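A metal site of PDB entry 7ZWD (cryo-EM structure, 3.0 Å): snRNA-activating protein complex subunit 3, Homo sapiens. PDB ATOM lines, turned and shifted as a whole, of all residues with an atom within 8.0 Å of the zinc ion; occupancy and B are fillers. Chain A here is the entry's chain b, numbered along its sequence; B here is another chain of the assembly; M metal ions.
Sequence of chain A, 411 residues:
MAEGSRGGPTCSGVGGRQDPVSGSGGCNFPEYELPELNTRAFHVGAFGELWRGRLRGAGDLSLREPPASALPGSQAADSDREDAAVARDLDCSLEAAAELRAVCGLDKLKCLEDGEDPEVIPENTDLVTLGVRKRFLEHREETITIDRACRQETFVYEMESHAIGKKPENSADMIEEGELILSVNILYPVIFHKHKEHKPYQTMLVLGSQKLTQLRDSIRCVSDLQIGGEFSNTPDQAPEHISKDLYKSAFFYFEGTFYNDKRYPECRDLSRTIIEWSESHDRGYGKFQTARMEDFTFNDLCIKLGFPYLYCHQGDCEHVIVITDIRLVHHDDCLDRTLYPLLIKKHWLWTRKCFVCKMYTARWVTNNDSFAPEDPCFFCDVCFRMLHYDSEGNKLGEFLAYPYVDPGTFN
The side-chain sulfur (SG) of Cys 354 sits close to the backbone NH (N) of Val 356.
The backbone NH (N) of Cys 354 sits at hydrogen-bond distance from the backbone carbonyl oxygen (O) of Tyr 360.
The side-chain amide nitrogen of Gln 338 of chain B sits close to the side-chain sulfur of Cys 383 (3.2 Å).
Four residues have an atom within 4 Å of the zinc ion: Cys 354, Cys 357, Cys 380 and Cys 383.
The nearest printed residue that does not touch the zinc ion is Val 356 (4.5 Å).
The zinc ion is bound by the side-chain sulfur (SG) of Cys 354 (2.1 Å), the side-chain sulfur (SG) of Cys 383 (2.2 Å), the side-chain sulfur (SG) of Cys 380 (2.2 Å) and the side-chain sulfur (SG) of Cys 357 (2.5 Å).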
ATOM      1  N   LYS A 353     -15.597 -15.358  19.594  1.00  0.00           N
ATOM      2  CA  LYS A 353     -16.069 -14.268  20.423  1.00  0.00           C
ATOM      3  C   LYS A 353     -17.579 -14.180  20.387  1.00  0.00           C
ATOM      4  O   LYS A 353     -18.235 -14.758  19.523  1.00  0.00           O
ATOM      5  CB  LYS A 353     -15.453 -12.933  19.970  1.00  0.00           C
ATOM      6  CG  LYS A 353     -13.982 -12.819  20.235  1.00  0.00           C
ATOM      7  CD  LYS A 353     -13.634 -11.393  20.534  1.00  0.00           C
ATOM      8  CE  LYS A 353     -12.212 -11.085  20.140  1.00  0.00           C
ATOM      9  NZ  LYS A 353     -12.030 -11.283  18.687  1.00  0.00           N
ATOM     10  N   CYS A 354     -18.123 -13.448  21.351  1.00  0.00           N
ATOM     11  CA  CYS A 354     -19.549 -13.156  21.349  1.00  0.00           C
ATOM     12  C   CYS A 354     -19.928 -12.493  20.040  1.00  0.00           C
ATOM     13  O   CYS A 354     -19.247 -11.601  19.548  1.00  0.00           O
ATOM     14  CB  CYS A 354     -19.898 -12.242  22.522  1.00  0.00           C
ATOM     15  SG  CYS A 354     -21.531 -11.528  22.424  1.00  0.00           S
ATOM     16  N   PHE A 355     -21.028 -12.951  19.463  1.00  0.00           N
ATOM     17  CA  PHE A 355     -21.431 -12.444  18.162  1.00  0.00           C
ATOM     18  C   PHE A 355     -22.080 -11.075  18.251  1.00  0.00           C
ATOM     19  O   PHE A 355     -22.058 -10.343  17.253  1.00  0.00           O
ATOM     20  CB  PHE A 355     -22.380 -13.408  17.477  1.00  0.00           C
ATOM     21  CG  PHE A 355     -21.688 -14.473  16.697  1.00  0.00           C
ATOM     22  CD1 PHE A 355     -20.349 -14.726  16.896  1.00  0.00           C
ATOM     23  CD2 PHE A 355     -22.361 -15.207  15.759  1.00  0.00           C
ATOM     24  CE1 PHE A 355     -19.708 -15.710  16.184  1.00  0.00           C
ATOM     25  CE2 PHE A 355     -21.720 -16.191  15.047  1.00  0.00           C
ATOM     26  CZ  PHE A 355     -20.392 -16.442  15.254  1.00  0.00           C
ATOM     27  N   VAL A 356     -22.638 -10.710  19.391  1.00  0.00           N
ATOM     28  CA  VAL A 356     -23.266  -9.412  19.554  1.00  0.00           C
ATOM     29  C   VAL A 356     -22.227  -8.329  19.760  1.00  0.00           C
ATOM     30  O   VAL A 356     -22.058  -7.445  18.925  1.00  0.00           O
ATOM     31  CB  VAL A 356     -24.265  -9.448  20.727  1.00  0.00           C
ATOM     32  CG1 VAL A 356     -24.876  -8.101  20.892  1.00  0.00           C
ATOM     33  CG2 VAL A 356     -25.323 -10.471  20.476  1.00  0.00           C
ATOM     34  N   CYS A 357     -21.486  -8.397  20.860  1.00  0.00           N
ATOM     35  CA  CYS A 357     -20.322  -7.553  21.067  1.00  0.00           C
ATOM     36  C   CYS A 357     -19.092  -8.428  20.929  1.00  0.00           C
ATOM     37  O   CYS A 357     -19.029  -9.534  21.468  1.00  0.00           O
ATOM     38  CB  CYS A 357     -20.329  -6.897  22.446  1.00  0.00           C
ATOM     39  SG  CYS A 357     -20.125  -8.038  23.815  1.00  0.00           S
ATOM     40  N   LYS A 358     -18.114  -7.932  20.202  1.00  0.00           N
ATOM     41  CA  LYS A 358     -16.907  -8.707  19.933  1.00  0.00           C
ATOM     42  C   LYS A 358     -15.835  -8.446  20.976  1.00  0.00           C
ATOM     43  O   LYS A 358     -14.646  -8.478  20.647  1.00  0.00           O
ATOM     44  CB  LYS A 358     -16.391  -8.399  18.539  1.00  0.00           C
ATOM     45  CG  LYS A 358     -17.442  -8.452  17.478  1.00  0.00           C
ATOM     46  CD  LYS A 358     -17.785  -9.877  17.128  1.00  0.00           C
ATOM     47  CE  LYS A 358     -18.964  -9.915  16.180  1.00  0.00           C
ATOM     48  NZ  LYS A 358     -18.779  -9.011  15.019  1.00  0.00           N
ATOM     49  N   MET A 359     -16.223  -8.173  22.215  1.00  0.00           N
ATOM     50  CA  MET A 359     -15.249  -7.879  23.255  1.00  0.00           C
ATOM     51  C   MET A 359     -14.942  -9.074  24.137  1.00  0.00           C
ATOM     52  O   MET A 359     -13.840  -9.144  24.686  1.00  0.00           O
ATOM     53  CB  MET A 359     -15.740  -6.719  24.124  1.00  0.00           C
ATOM     54  CG  MET A 359     -16.057  -5.466  23.345  1.00  0.00           C
ATOM     55  SD  MET A 359     -14.750  -5.091  22.163  1.00  0.00           S
ATOM     56  CE  MET A 359     -15.466  -3.700  21.288  1.00  0.00           C
ATOM     57  N   TYR A 360     -15.876 -10.007  24.301  1.00  0.00           N
ATOM     58  CA  TYR A 360     -15.672 -11.141  25.174  1.00  0.00           C
ATOM     59  C   TYR A 360     -15.775 -12.425  24.380  1.00  0.00           C
ATOM     60  O   TYR A 360     -16.280 -12.453  23.268  1.00  0.00           O
ATOM     61  CB  TYR A 360     -16.682 -11.161  26.317  1.00  0.00           C
ATOM     62  CG  TYR A 360     -16.730  -9.880  27.090  1.00  0.00           C
ATOM     63  CD1 TYR A 360     -15.675  -9.486  27.885  1.00  0.00           C
ATOM     64  CD2 TYR A 360     -17.838  -9.063  27.035  1.00  0.00           C
ATOM     65  CE1 TYR A 360     -15.715  -8.319  28.586  1.00  0.00           C
ATOM     66  CE2 TYR A 360     -17.888  -7.892  27.745  1.00  0.00           C
ATOM     67  CZ  TYR A 360     -16.827  -7.530  28.514  1.00  0.00           C
ATOM     68  OH  TYR A 360     -16.864  -6.356  29.228  1.00  0.00           O
ATOM     69  N   THR A 361     -15.276 -13.498  24.971  1.00  0.00           N
ATOM     70  CA  THR A 361     -15.310 -14.785  24.294  1.00  0.00           C
ATOM     71  C   THR A 361     -16.670 -15.432  24.470  1.00  0.00           C
ATOM     72  O   THR A 361     -17.464 -15.034  25.320  1.00  0.00           O
ATOM     73  CB  THR A 361     -14.241 -15.714  24.829  1.00  0.00           C
ATOM     74  OG1 THR A 361     -14.155 -16.865  23.985  1.00  0.00           O
ATOM     75  CG2 THR A 361     -14.605 -16.164  26.206  1.00  0.00           C
ATOM     76  N   ALA A 362     -16.913 -16.442  23.669  1.00  0.00           N
ATOM     77  CA  ALA A 362     -18.194 -17.119  23.678  1.00  0.00           C
ATOM     78  C   ALA A 362     -18.292 -18.113  24.818  1.00  0.00           C
ATOM     79  O   ALA A 362     -17.510 -19.061  24.898  1.00  0.00           O
ATOM     80  CB  ALA A 362     -18.396 -17.841  22.359  1.00  0.00           C
ATOM     81  N   PHE A 378     -22.873 -17.702  18.886  1.00  0.00           N
ATOM     82  CA  PHE A 378     -22.075 -17.755  20.104  1.00  0.00           C
ATOM     83  C   PHE A 378     -22.208 -16.442  20.856  1.00  0.00           C
ATOM     84  O   PHE A 378     -22.146 -15.368  20.263  1.00  0.00           O
ATOM     85  CB  PHE A 378     -20.611 -18.013  19.767  1.00  0.00           C
ATOM     86  CG  PHE A 378     -20.392 -19.214  18.918  1.00  0.00           C
ATOM     87  CD1 PHE A 378     -20.203 -20.438  19.491  1.00  0.00           C
ATOM     88  CD2 PHE A 378     -20.375 -19.108  17.562  1.00  0.00           C
ATOM     89  CE1 PHE A 378     -19.997 -21.534  18.712  1.00  0.00           C
ATOM     90  CE2 PHE A 378     -20.169 -20.204  16.783  1.00  0.00           C
ATOM     91  CZ  PHE A 378     -19.986 -21.416  17.367  1.00  0.00           C
ATOM     92  N   PHE A 379     -22.366 -16.537  22.165  1.00  0.00           N
ATOM     93  CA  PHE A 379     -22.545 -15.367  23.005  1.00  0.00           C
ATOM     94  C   PHE A 379     -21.633 -15.446  24.210  1.00  0.00           C
ATOM     95  O   PHE A 379     -21.253 -16.524  24.652  1.00  0.00           O
ATOM     96  CB  PHE A 379     -23.979 -15.249  23.509  1.00  0.00           C
ATOM     97  CG  PHE A 379     -24.992 -15.186  22.426  1.00  0.00           C
ATOM     98  CD1 PHE A 379     -25.407 -13.981  21.908  1.00  0.00           C
ATOM     99  CD2 PHE A 379     -25.569 -16.339  21.935  1.00  0.00           C
ATOM    100  CE1 PHE A 379     -26.349 -13.919  20.932  1.00  0.00           C
ATOM    101  CE2 PHE A 379     -26.510 -16.276  20.950  1.00  0.00           C
ATOM    102  CZ  PHE A 379     -26.900 -15.066  20.449  1.00  0.00           C
ATOM    103  N   CYS A 380     -21.269 -14.274  24.724  1.00  0.00           N
ATOM    104  CA  CYS A 380     -20.704 -14.192  26.056  1.00  0.00           C
ATOM    105  C   CYS A 380     -21.829 -14.345  27.067  1.00  0.00           C
ATOM    106  O   CYS A 380     -22.988 -14.538  26.706  1.00  0.00           O
ATOM    107  CB  CYS A 380     -19.949 -12.883  26.249  1.00  0.00           C
ATOM    108  SG  CYS A 380     -20.876 -11.413  25.783  1.00  0.00           S
ATOM    109  N   ASP A 381     -21.491 -14.260  28.344  1.00  0.00           N
ATOM    110  CA  ASP A 381     -22.544 -14.391  29.343  1.00  0.00           C
ATOM    111  C   ASP A 381     -23.445 -13.162  29.345  1.00  0.00           C
ATOM    112  O   ASP A 381     -24.673 -13.284  29.470  1.00  0.00           O
ATOM    113  CB  ASP A 381     -21.935 -14.600  30.722  1.00  0.00           C
ATOM    114  CG  ASP A 381     -22.838 -15.390  31.647  1.00  0.00           C
ATOM    115  OD1 ASP A 381     -23.167 -16.538  31.300  1.00  0.00           O
ATOM    116  OD2 ASP A 381     -23.223 -14.847  32.700  1.00  0.00           O
ATOM    117  N   VAL A 382     -22.865 -11.980  29.188  1.00  0.00           N
ATOM    118  CA  VAL A 382     -23.650 -10.747  29.234  1.00  0.00           C
ATOM    119  C   VAL A 382     -24.662 -10.707  28.106  1.00  0.00           C
ATOM    120  O   VAL A 382     -25.872 -10.587  28.343  1.00  0.00           O
ATOM    121  CB  VAL A 382     -22.717  -9.526  29.186  1.00  0.00           C
ATOM    122  CG1 VAL A 382     -23.510  -8.268  29.360  1.00  0.00           C
ATOM    123  CG2 VAL A 382     -21.647  -9.637  30.240  1.00  0.00           C
ATOM    124  N   CYS A 383     -24.188 -10.816  26.872  1.00  0.00           N
ATOM    125  CA  CYS A 383     -25.094 -10.737  25.731  1.00  0.00           C
ATOM    126  C   CYS A 383     -26.045 -11.908  25.650  1.00  0.00           C
ATOM    127  O   CYS A 383     -27.051 -11.836  24.954  1.00  0.00           O
ATOM    128  CB  CYS A 383     -24.286 -10.627  24.441  1.00  0.00           C
ATOM    129  SG  CYS A 383     -23.184  -9.219  24.400  1.00  0.00           S
ATOM    130  N   PHE A 384     -25.742 -13.004  26.332  1.00  0.00           N
ATOM    131  CA  PHE A 384     -26.698 -14.106  26.388  1.00  0.00           C
ATOM    132  C   PHE A 384     -27.824 -13.796  27.363  1.00  0.00           C
ATOM    133  O   PHE A 384     -29.000 -13.916  27.032  1.00  0.00           O
ATOM    134  CB  PHE A 384     -25.978 -15.382  26.797  1.00  0.00           C
ATOM    135  CG  PHE A 384     -26.861 -16.576  26.860  1.00  0.00           C
ATOM    136  CD1 PHE A 384     -27.250 -17.218  25.706  1.00  0.00           C
ATOM    137  CD2 PHE A 384     -27.289 -17.058  28.073  1.00  0.00           C
ATOM    138  CE1 PHE A 384     -28.058 -18.324  25.770  1.00  0.00           C
ATOM    139  CE2 PHE A 384     -28.097 -18.165  28.137  1.00  0.00           C
ATOM    140  CZ  PHE A 384     -28.481 -18.798  26.985  1.00  0.00           C
ATOM    141  N   MET A 386     -28.824 -10.975  28.311  1.00  0.00           N
ATOM    142  CA  MET A 386     -29.547  -9.777  27.927  1.00  0.00           C
ATOM    143  C   MET A 386     -30.492 -10.002  26.762  1.00  0.00           C
ATOM    144  O   MET A 386     -31.436  -9.221  26.597  1.00  0.00           O
ATOM    145  CB  MET A 386     -28.568  -8.663  27.557  1.00  0.00           C
ATOM    146  CG  MET A 386     -27.854  -8.061  28.738  1.00  0.00           C
ATOM    147  SD  MET A 386     -26.777  -6.724  28.232  1.00  0.00           S
ATOM    148  CE  MET A 386     -27.937  -5.726  27.329  1.00  0.00           C
ATOM    149  N   LEU B 334     -29.611  -4.891  20.026  1.00  0.00           N
ATOM    150  CA  LEU B 334     -28.678  -5.248  21.089  1.00  0.00           C
ATOM    151  C   LEU B 334     -27.237  -5.011  20.655  1.00  0.00           C
ATOM    152  O   LEU B 334     -26.408  -4.546  21.448  1.00  0.00           O
ATOM    153  CB  LEU B 334     -28.870  -6.702  21.490  1.00  0.00           C
ATOM    154  CG  LEU B 334     -27.881  -7.225  22.522  1.00  0.00           C
ATOM    155  CD1 LEU B 334     -28.127  -6.529  23.829  1.00  0.00           C
ATOM    156  CD2 LEU B 334     -28.042  -8.704  22.675  1.00  0.00           C
ATOM    157  N   GLN B 338     -24.669  -2.508  22.599  1.00  0.00           N
ATOM    158  CA  GLN B 338     -23.386  -2.920  23.151  1.00  0.00           C
ATOM    159  C   GLN B 338     -22.242  -2.113  22.537  1.00  0.00           C
ATOM    160  O   GLN B 338     -21.456  -1.495  23.258  1.00  0.00           O
ATOM    161  CB  GLN B 338     -23.166  -4.413  22.983  1.00  0.00           C
ATOM    162  CG  GLN B 338     -24.215  -5.248  23.663  1.00  0.00           C
ATOM    163  CD  GLN B 338     -24.058  -5.279  25.151  1.00  0.00           C
ATOM    164  OE1 GLN B 338     -24.538  -4.397  25.855  1.00  0.00           O
ATOM    165  NE2 GLN B 338     -23.403  -6.319  25.655  1.00  0.00           N
ATOM    166  N   GLN B 339     -22.169  -2.084  21.209  1.00  0.00           N
ATOM    167  CA  GLN B 339     -21.088  -1.348  20.559  1.00  0.00           C
ATOM    168  C   GLN B 339     -21.110   0.131  20.908  1.00  0.00           C
ATOM    169  O   GLN B 339     -20.144   0.842  20.594  1.00  0.00           O
ATOM    170  CB  GLN B 339     -21.165  -1.520  19.038  1.00  0.00           C
ATOM    171  CG  GLN B 339     -20.960  -2.945  18.559  1.00  0.00           C
ATOM    172  CD  GLN B 339     -19.720  -3.598  19.160  1.00  0.00           C
ATOM    173  OE1 GLN B 339     -19.800  -4.310  20.160  1.00  0.00           O
ATOM    174  NE2 GLN B 339     -18.574  -3.374  18.539  1.00  0.00           N
ATOM    175  N   LEU B 344     -19.965  -1.924  29.533  1.00  0.00           N
ATOM    176  CA  LEU B 344     -19.585  -3.238  29.027  1.00  0.00           C
ATOM    177  C   LEU B 344     -18.309  -3.725  29.678  1.00  0.00           C
ATOM    178  O   LEU B 344     -18.239  -4.845  30.174  1.00  0.00           O
ATOM    179  CB  LEU B 344     -19.438  -3.171  27.514  1.00  0.00           C
ATOM    180  CG  LEU B 344     -19.287  -4.506  26.802  1.00  0.00           C
ATOM    181  CD1 LEU B 344     -20.526  -5.337  27.008  1.00  0.00           C
ATOM    182  CD2 LEU B 344     -19.024  -4.279  25.331  1.00  0.00           C
HETATM  183 ZN    ZN M   1     -21.287 -10.187  24.014  1.00  0.00          ZN
